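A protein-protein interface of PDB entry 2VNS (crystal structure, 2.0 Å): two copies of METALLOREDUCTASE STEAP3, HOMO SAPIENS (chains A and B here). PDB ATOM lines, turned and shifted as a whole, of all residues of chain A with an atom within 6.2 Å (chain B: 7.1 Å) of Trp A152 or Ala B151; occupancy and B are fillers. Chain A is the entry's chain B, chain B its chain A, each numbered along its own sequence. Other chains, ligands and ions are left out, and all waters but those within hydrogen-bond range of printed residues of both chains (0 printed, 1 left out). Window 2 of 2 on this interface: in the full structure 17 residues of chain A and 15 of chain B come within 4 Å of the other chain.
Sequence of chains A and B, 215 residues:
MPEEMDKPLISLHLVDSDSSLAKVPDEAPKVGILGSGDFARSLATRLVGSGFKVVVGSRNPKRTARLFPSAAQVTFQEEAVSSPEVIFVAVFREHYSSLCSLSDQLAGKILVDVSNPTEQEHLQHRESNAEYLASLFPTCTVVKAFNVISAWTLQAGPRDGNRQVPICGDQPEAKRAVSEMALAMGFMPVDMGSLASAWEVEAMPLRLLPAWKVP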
ATOM      1  N   SER A  42       3.672   2.128  14.462  1.00  0.00           N
ATOM      2  CA  SER A  42       2.256   2.458  14.687  1.00  0.00           C
ATOM      3  C   SER A  42       1.734   3.456  13.635  1.00  0.00           C
ATOM      4  O   SER A  42       0.623   3.293  13.100  1.00  0.00           O
ATOM      5  CB  SER A  42       2.063   2.986  16.114  1.00  0.00           C
ATOM      6  OG  SER A  42       2.516   2.034  17.076  1.00  0.00           O
ATOM      7  N   SER A 150      -0.761   8.946  21.259  1.00  0.00           N
ATOM      8  CA  SER A 150       0.027   7.768  21.658  1.00  0.00           C
ATOM      9  C   SER A 150       0.129   6.767  20.508  1.00  0.00           C
ATOM     10  O   SER A 150      -0.728   6.737  19.599  1.00  0.00           O
ATOM     11  CB  SER A 150      -0.585   7.057  22.860  1.00  0.00           C
ATOM     12  OG  SER A 150      -1.769   6.369  22.489  1.00  0.00           O
ATOM     13  N   ALA A 151       1.177   5.953  20.570  1.00  0.00           N
ATOM     14  CA  ALA A 151       1.416   4.889  19.616  1.00  0.00           C
ATOM     15  C   ALA A 151       0.226   3.942  19.571  1.00  0.00           C
ATOM     16  O   ALA A 151      -0.202   3.552  18.497  1.00  0.00           O
ATOM     17  CB  ALA A 151       2.715   4.119  19.964  1.00  0.00           C
ATOM     18  N   TRP A 152      -0.349   3.608  20.721  1.00  0.00           N
ATOM     19  CA  TRP A 152      -1.504   2.703  20.704  1.00  0.00           C
ATOM     20  C   TRP A 152      -2.752   3.348  20.091  1.00  0.00           C
ATOM     21  O   TRP A 152      -3.573   2.636  19.482  1.00  0.00           O
ATOM     22  CB  TRP A 152      -1.804   2.106  22.080  1.00  0.00           C
ATOM     23  CG  TRP A 152      -2.934   1.092  21.989  1.00  0.00           C
ATOM     24  CD1 TRP A 152      -4.181   1.190  22.554  1.00  0.00           C
ATOM     25  CD2 TRP A 152      -2.933  -0.126  21.235  1.00  0.00           C
ATOM     26  NE1 TRP A 152      -4.935   0.089  22.223  1.00  0.00           N
ATOM     27  CE2 TRP A 152      -4.194  -0.729  21.411  1.00  0.00           C
ATOM     28  CE3 TRP A 152      -1.984  -0.775  20.438  1.00  0.00           C
ATOM     29  CZ2 TRP A 152      -4.529  -1.938  20.810  1.00  0.00           C
ATOM     30  CZ3 TRP A 152      -2.323  -1.994  19.851  1.00  0.00           C
ATOM     31  CH2 TRP A 152      -3.583  -2.551  20.040  1.00  0.00           C
ATOM     32  N   THR A 153      -2.887   4.673  20.219  1.00  0.00           N
ATOM     33  CA  THR A 153      -4.005   5.398  19.589  1.00  0.00           C
ATOM     34  C   THR A 153      -3.894   5.349  18.069  1.00  0.00           C
ATOM     35  O   THR A 153      -4.899   5.170  17.377  1.00  0.00           O
ATOM     36  CB  THR A 153      -4.073   6.844  20.044  1.00  0.00           C
ATOM     37  OG1 THR A 153      -4.363   6.855  21.437  1.00  0.00           O
ATOM     38  CG2 THR A 153      -5.174   7.625  19.295  1.00  0.00           C
ATOM     39  N   LEU A 154      -2.674   5.468  17.568  1.00  0.00           N
ATOM     40  CA  LEU A 154      -2.405   5.262  16.163  1.00  0.00           C
ATOM     41  C   LEU A 154      -2.743   3.859  15.707  1.00  0.00           C
ATOM     42  O   LEU A 154      -3.366   3.679  14.674  1.00  0.00           O
ATOM     43  CB  LEU A 154      -0.950   5.592  15.821  1.00  0.00           C
ATOM     44  CG  LEU A 154      -0.581   7.067  15.788  1.00  0.00           C
ATOM     45  CD1 LEU A 154       0.923   7.204  15.776  1.00  0.00           C
ATOM     46  CD2 LEU A 154      -1.197   7.764  14.569  1.00  0.00           C
ATOM     47  N   GLN A 155      -2.366   2.873  16.492  1.00  0.00           N
ATOM     48  CA  GLN A 155      -2.617   1.479  16.154  1.00  0.00           C
ATOM     49  C   GLN A 155      -4.083   1.110  16.200  1.00  0.00           C
ATOM     50  O   GLN A 155      -4.612   0.561  15.246  1.00  0.00           O
ATOM     51  CB  GLN A 155      -1.907   0.589  17.143  1.00  0.00           C
ATOM     52  CG  GLN A 155      -0.431   0.685  17.053  1.00  0.00           C
ATOM     53  CD  GLN A 155       0.200  -0.532  16.479  1.00  0.00           C
ATOM     54  OE1 GLN A 155      -0.469  -1.504  16.142  1.00  0.00           O
ATOM     55  NE2 GLN A 155       1.490  -0.494  16.363  1.00  0.00           N
ATOM     56  N   ALA A 156      -4.718   1.411  17.319  1.00  0.00           N
ATOM     57  CA  ALA A 156      -6.045   0.888  17.608  1.00  0.00           C
ATOM     58  C   ALA A 156      -7.080   1.956  17.408  1.00  0.00           C
ATOM     59  O   ALA A 156      -8.063   1.725  16.717  1.00  0.00           O
ATOM     60  CB  ALA A 156      -6.121   0.379  19.005  1.00  0.00           C
ATOM     61  N   GLY A 157      -6.826   3.126  18.005  1.00  0.00           N
ATOM     62  CA  GLY A 157      -7.830   4.179  18.206  1.00  0.00           C
ATOM     63  C   GLY A 157      -8.164   4.822  16.889  1.00  0.00           C
ATOM     64  O   GLY A 157      -8.513   4.129  15.959  1.00  0.00           O
ATOM     65  N   ASP B  38      -6.893  -6.553  16.665  1.00  0.00           N
ATOM     66  CA  ASP B  38      -5.794  -5.852  17.337  1.00  0.00           C
ATOM     67  C   ASP B  38      -4.996  -6.786  18.223  1.00  0.00           C
ATOM     68  O   ASP B  38      -3.769  -6.732  18.259  1.00  0.00           O
ATOM     69  CB  ASP B  38      -6.314  -4.699  18.179  1.00  0.00           C
ATOM     70  CG  ASP B  38      -6.779  -3.522  17.346  1.00  0.00           C
ATOM     71  OD1 ASP B  38      -6.275  -3.300  16.225  1.00  0.00           O
ATOM     72  OD2 ASP B  38      -7.670  -2.821  17.833  1.00  0.00           O
ATOM     73  N   PHE B  39      -5.687  -7.646  18.949  1.00  0.00           N
ATOM     74  CA  PHE B  39      -4.982  -8.626  19.803  1.00  0.00           C
ATOM     75  C   PHE B  39      -4.190  -9.682  19.024  1.00  0.00           C
ATOM     76  O   PHE B  39      -3.022  -9.939  19.353  1.00  0.00           O
ATOM     77  CB  PHE B  39      -5.912  -9.296  20.791  1.00  0.00           C
ATOM     78  CG  PHE B  39      -5.174  -9.905  21.961  1.00  0.00           C
ATOM     79  CD1 PHE B  39      -4.768  -9.119  23.014  1.00  0.00           C
ATOM     80  CD2 PHE B  39      -4.878 -11.249  21.999  1.00  0.00           C
ATOM     81  CE1 PHE B  39      -4.084  -9.666  24.090  1.00  0.00           C
ATOM     82  CE2 PHE B  39      -4.205 -11.795  23.121  1.00  0.00           C
ATOM     83  CZ  PHE B  39      -3.817 -10.992  24.129  1.00  0.00           C
ATOM     84  N   ALA B  40      -4.809 -10.278  18.003  1.00  0.00           N
ATOM     85  CA  ALA B  40      -4.139 -11.205  17.073  1.00  0.00           C
ATOM     86  C   ALA B  40      -2.844 -10.526  16.597  1.00  0.00           C
ATOM     87  O   ALA B  40      -1.801 -11.160  16.474  1.00  0.00           O
ATOM     88  CB  ALA B  40      -5.079 -11.624  15.932  1.00  0.00           C
ATOM     89  N   ARG B  41      -2.913  -9.255  16.264  1.00  0.00           N
ATOM     90  CA  ARG B  41      -1.947  -8.630  15.380  1.00  0.00           C
ATOM     91  C   ARG B  41      -0.771  -8.348  16.358  1.00  0.00           C
ATOM     92  O   ARG B  41       0.412  -8.501  16.038  1.00  0.00           O
ATOM     93  CB  ARG B  41      -2.511  -7.319  14.854  1.00  0.00           C
ATOM     94  CG  ARG B  41      -1.582  -6.578  13.935  1.00  0.00           C
ATOM     95  CD  ARG B  41      -2.341  -5.566  13.141  1.00  0.00           C
ATOM     96  NE  ARG B  41      -3.061  -4.637  14.013  1.00  0.00           N
ATOM     97  CZ  ARG B  41      -2.468  -3.695  14.710  1.00  0.00           C
ATOM     98  NH1 ARG B  41      -1.169  -3.566  14.605  1.00  0.00           N
ATOM     99  NH2 ARG B  41      -3.164  -2.888  15.498  1.00  0.00           N
ATOM    100  N   SER B  42      -1.122  -7.949  17.578  1.00  0.00           N
ATOM    101  CA  SER B  42      -0.145  -7.662  18.634  1.00  0.00           C
ATOM    102  C   SER B  42       0.584  -8.929  19.108  1.00  0.00           C
ATOM    103  O   SER B  42       1.795  -8.942  19.260  1.00  0.00           O
ATOM    104  CB  SER B  42      -0.844  -6.985  19.789  1.00  0.00           C
ATOM    105  OG  SER B  42      -1.327  -5.743  19.352  1.00  0.00           O
ATOM    106  N   LEU B  43      -0.169 -10.002  19.293  1.00  0.00           N
ATOM    107  CA  LEU B  43       0.393 -11.315  19.611  1.00  0.00           C
ATOM    108  C   LEU B  43       1.383 -11.743  18.525  1.00  0.00           C
ATOM    109  O   LEU B  43       2.503 -12.220  18.834  1.00  0.00           O
ATOM    110  CB  LEU B  43      -0.708 -12.381  19.697  1.00  0.00           C
ATOM    111  CG  LEU B  43      -1.371 -12.773  21.005  1.00  0.00           C
ATOM    112  CD1 LEU B  43      -2.452 -13.860  20.676  1.00  0.00           C
ATOM    113  CD2 LEU B  43      -0.337 -13.284  22.007  1.00  0.00           C
ATOM    114  N   ILE B 149      -3.115  -9.374  29.775  1.00  0.00           N
ATOM    115  CA  ILE B 149      -2.069  -8.634  29.059  1.00  0.00           C
ATOM    116  C   ILE B 149      -2.718  -7.803  27.961  1.00  0.00           C
ATOM    117  O   ILE B 149      -3.440  -8.338  27.124  1.00  0.00           O
ATOM    118  CB  ILE B 149      -1.046  -9.614  28.444  1.00  0.00           C
ATOM    119  CG1 ILE B 149      -0.442 -10.542  29.523  1.00  0.00           C
ATOM    120  CG2 ILE B 149       0.059  -8.870  27.724  1.00  0.00           C
ATOM    121  CD1 ILE B 149       0.319  -9.826  30.634  1.00  0.00           C
ATOM    122  N   SER B 150      -2.487  -6.496  27.973  1.00  0.00           N
ATOM    123  CA  SER B 150      -3.058  -5.617  26.941  1.00  0.00           C
ATOM    124  C   SER B 150      -2.356  -5.808  25.605  1.00  0.00           C
ATOM    125  O   SER B 150      -1.183  -6.229  25.558  1.00  0.00           O
ATOM    126  CB  SER B 150      -2.927  -4.168  27.348  1.00  0.00           C
ATOM    127  OG  SER B 150      -1.559  -3.788  27.351  1.00  0.00           O
ATOM    128  N   ALA B 151      -3.059  -5.462  24.529  1.00  0.00           N
ATOM    129  CA  ALA B 151      -2.496  -5.533  23.187  1.00  0.00           C
ATOM    130  C   ALA B 151      -1.237  -4.657  23.072  1.00  0.00           C
ATOM    131  O   ALA B 151      -0.248  -5.057  22.457  1.00  0.00           O
ATOM    132  CB  ALA B 151      -3.556  -5.139  22.137  1.00  0.00           C
ATOM    133  N   TRP B 152      -1.240  -3.485  23.698  1.00  0.00           N
ATOM    134  CA  TRP B 152      -0.062  -2.609  23.632  1.00  0.00           C
ATOM    135  C   TRP B 152       1.118  -3.192  24.398  1.00  0.00           C
ATOM    136  O   TRP B 152       2.273  -3.016  23.999  1.00  0.00           O
ATOM    137  CB  TRP B 152      -0.368  -1.194  24.115  1.00  0.00           C
ATOM    138  CG  TRP B 152       0.848  -0.300  23.944  1.00  0.00           C
ATOM    139  CD1 TRP B 152       1.547   0.335  24.918  1.00  0.00           C
ATOM    140  CD2 TRP B 152       1.525  -0.025  22.717  1.00  0.00           C
ATOM    141  NE1 TRP B 152       2.620   1.007  24.373  1.00  0.00           N
ATOM    142  CE2 TRP B 152       2.625   0.801  23.021  1.00  0.00           C
ATOM    143  CE3 TRP B 152       1.304  -0.391  21.382  1.00  0.00           C
ATOM    144  CZ2 TRP B 152       3.490   1.270  22.045  1.00  0.00           C
ATOM    145  CZ3 TRP B 152       2.172   0.066  20.419  1.00  0.00           C
ATOM    146  CH2 TRP B 152       3.251   0.886  20.754  1.00  0.00           C
ATOM    147  N   THR B 153       0.840  -3.887  25.497  1.00  0.00           N
ATOM    148  CA  THR B 153       1.911  -4.554  26.266  1.00  0.00           C
ATOM    149  C   THR B 153       2.567  -5.623  25.413  1.00  0.00           C
ATOM    150  O   THR B 153       3.781  -5.812  25.470  1.00  0.00           O
ATOM    151  CB  THR B 153       1.378  -5.206  27.553  1.00  0.00           C
ATOM    152  OG1 THR B 153       0.855  -4.201  28.405  1.00  0.00           O
ATOM    153  CG2 THR B 153       2.474  -5.985  28.310  1.00  0.00           C
ATOM    154  N   LEU B 154       1.762  -6.326  24.630  1.00  0.00           N
ATOM    155  CA  LEU B 154       2.289  -7.287  23.647  1.00  0.00           C
ATOM    156  C   LEU B 154       3.152  -6.603  22.588  1.00  0.00           C
ATOM    157  O   LEU B 154       4.228  -7.088  22.254  1.00  0.00           O
ATOM    158  CB  LEU B 154       1.160  -8.070  22.981  1.00  0.00           C
ATOM    159  CG  LEU B 154       0.630  -9.258  23.793  1.00  0.00           C
ATOM    160  CD1 LEU B 154      -0.547  -9.918  23.081  1.00  0.00           C
ATOM    161  CD2 LEU B 154       1.736 -10.274  24.043  1.00  0.00           C
ATOM    162  N   GLN B 155       2.701  -5.456  22.105  1.00  0.00           N
ATOM    163  CA  GLN B 155       3.408  -4.710  21.072  1.00  0.00           C
ATOM    164  C   GLN B 155       4.698  -4.081  21.575  1.00  0.00           C
ATOM    165  O   GLN B 155       5.732  -4.170  20.938  1.00  0.00           O
ATOM    166  CB  GLN B 155       2.555  -3.564  20.582  1.00  0.00           C
ATOM    167  CG  GLN B 155       1.328  -3.968  19.858  1.00  0.00           C
ATOM    168  CD  GLN B 155       1.486  -3.854  18.403  1.00  0.00           C
ATOM    169  OE1 GLN B 155       2.484  -3.353  17.924  1.00  0.00           O
ATOM    170  NE2 GLN B 155       0.502  -4.313  17.677  1.00  0.00           N
ATOM    171  N   ALA B 156       4.590  -3.389  22.690  1.00  0.00           N
ATOM    172  CA  ALA B 156       5.640  -2.512  23.150  1.00  0.00           C
ATOM    173  C   ALA B 156       6.384  -3.165  24.266  1.00  0.00           C
ATOM    174  O   ALA B 156       7.596  -3.329  24.184  1.00  0.00           O
ATOM    175  CB  ALA B 156       5.057  -1.237  23.656  1.00  0.00           C
ATOM    176  N   GLY B 157       5.614  -3.550  25.292  1.00  0.00           N
ATOM    177  CA  GLY B 157       6.098  -3.867  26.642  1.00  0.00           C
ATOM    178  C   GLY B 157       6.838  -5.173  26.617  1.00  0.00           C
ATOM    179  O   GLY B 157       7.739  -5.318  25.820  1.00  0.00           O
ATOM    180  N   LEU B 206      -7.657  -6.505  33.455  1.00  0.00           N
ATOM    181  CA  LEU B 206      -6.690  -6.235  32.402  1.00  0.00           C
ATOM    182  C   LEU B 206      -5.706  -5.157  32.846  1.00  0.00           C
ATOM    183  O   LEU B 206      -6.090  -4.144  33.403  1.00  0.00           O
ATOM    184  CB  LEU B 206      -7.408  -5.788  31.125  1.00  0.00           C
ATOM    185  CG  LEU B 206      -6.553  -5.443  29.904  1.00  0.00           C
ATOM    186  CD1 LEU B 206      -5.769  -6.652  29.422  1.00  0.00           C
ATOM    187  CD2 LEU B 206      -7.451  -4.931  28.806  1.00  0.00           C
ATOM    188  N   ARG B 207      -4.476  -5.348  32.502  1.00  0.00           N
ATOM    189  CA  ARG B 207      -3.416  -4.449  32.936  1.00  0.00           C
ATOM    190  C   ARG B 207      -2.858  -3.639  31.775  1.00  0.00           C
ATOM    191  O   ARG B 207      -2.503  -4.196  30.740  1.00  0.00           O
ATOM    192  CB  ARG B 207      -2.281  -5.257  33.548  1.00  0.00           C
ATOM    193  CG  ARG B 207      -2.694  -6.121  34.712  1.00  0.00           C
ATOM    194  CD  ARG B 207      -3.122  -5.285  35.892  1.00  0.00           C
ATOM    195  NE  ARG B 207      -3.534  -6.114  37.016  1.00  0.00           N
ATOM    196  CZ  ARG B 207      -3.845  -5.635  38.211  1.00  0.00           C
ATOM    197  NH1 ARG B 207      -3.770  -4.335  38.448  1.00  0.00           N
ATOM    198  NH2 ARG B 207      -4.204  -6.467  39.178  1.00  0.00           N
ATOM    199  N   LEU B 208      -2.758  -2.355  31.938  1.00  0.00           N
ATOM    200  CA  LEU B 208      -1.941  -1.518  31.035  1.00  0.00           C
ATOM    201  C   LEU B 208      -0.513  -1.279  31.555  1.00  0.00           C
ATOM    202  O   LEU B 208      -0.301  -1.016  32.739  1.00  0.00           O
ATOM    203  CB  LEU B 208      -2.640  -0.175  30.769  1.00  0.00           C
ATOM    204  CG  LEU B 208      -4.143  -0.206  30.464  1.00  0.00           C
ATOM    205  CD1 LEU B 208      -4.546  -1.434  29.663  1.00  0.00           C
ATOM    206  CD2 LEU B 208      -4.966  -0.097  31.738  1.00  0.00           C
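The side-chain hydroxyl (OG) of Ser A42 lies within hydrogen-bond range of the side-chain amide nitrogen (NE2) of Gln A155, 2.8 Å away.
The backbone carbonyl oxygen (O) of Ala B151 lies close to the side-chain hydroxyl (OG) of Ser B42 (3.4 Å).
The backbone carbonyl oxygen of Asp B38 lies within hydrogen-bond range of the side-chain hydroxyl of Ser B42 (2.9 Å).
OG of Ser A42 sits close to O of Ala A151.
The side-chain amide nitrogen (NE2) of Gln B155 sits at hydrogen-bond distance from the side-chain hydroxyl (OG) of Ser B42, at 2.9 Å.
The guanidinium group (NH2) of Arg B41 is in salt-bridge range of the side-chain carboxylate (OD1) of Asp B38.
Of chain B, only Asp B38, Ser B42, Ala B151 and Trp B152 come within 4 Å of Trp A152.
Ala B151 touches just one residue of chain A: Trp A152 (3.3 Å).
Printed residues of chain A within 4 Å of Ser B42: Trp A152.
Of the printed residues of chain A, Asp B38 touches Trp A152 (3.9 Å) and Ala A156 (3.7 Å).
Printed residues of chain B within 4 Å of Ala A156: Asp B38.
Of the printed residues of chain B, Gln A155 touches Arg B41 and Gln B155.
Gly B157 touches none of the printed residues of chain A.
The nearest printed residue of chain A that does not touch Ala B151 is Ala A156 (6.8 Å).
The nearest printed residue of chain B that does not touch Ser A42 is Gln B155 (5.5 Å).
Ser A42 touches Trp B152.
Trp B152 touches Ala A151.
CH2 of Trp A152 touches CB of Asp B38 (3.9 Å).
Trp A152 touches Ser B42 (CZ3 to OG, 3.9 Å).
CH2 of Trp A152 touches CB of Ala B151, at 3.3 Å.
Trp B152 touches Trp A152.
Ala A156 touches Asp B38.
Hydrophobic or aromatic side chains of chain A within 4 Å of the printed part of chain B: Ala A151, Trp A152 and Ala A156.
Hydrophobic or aromatic side chains of chain B that line the printed part of chain A: Ala B151 and Trp B152.
Among the printed residues, 9 pairs touch across the chains.
Among the printed residues, no Asp or Glu carboxylate lies within 4 Å of a Lys or Arg side-chain nitrogen of the other chain.
Ser A42 touches Trp B152, and with the chains exchanged Trp A152 touches Ser B42.
Ala A151 touches Trp B152, and with the chains exchanged Trp A152 touches Ala B151.
Trp B152 touches its own counterpart, Trp A152.
Gln A155 touches its own counterpart, Gln B155.
9 positions are printed for both chains.
The guanidinium group of Arg B41 is in hydrogen-bond range of the side-chain amide oxygen of Gln A155 (2.7 Å).
The side-chain amide nitrogen of Gln B155 lies within hydrogen-bond range of the side-chain amide oxygen of Gln A155, 3.3 Å away.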
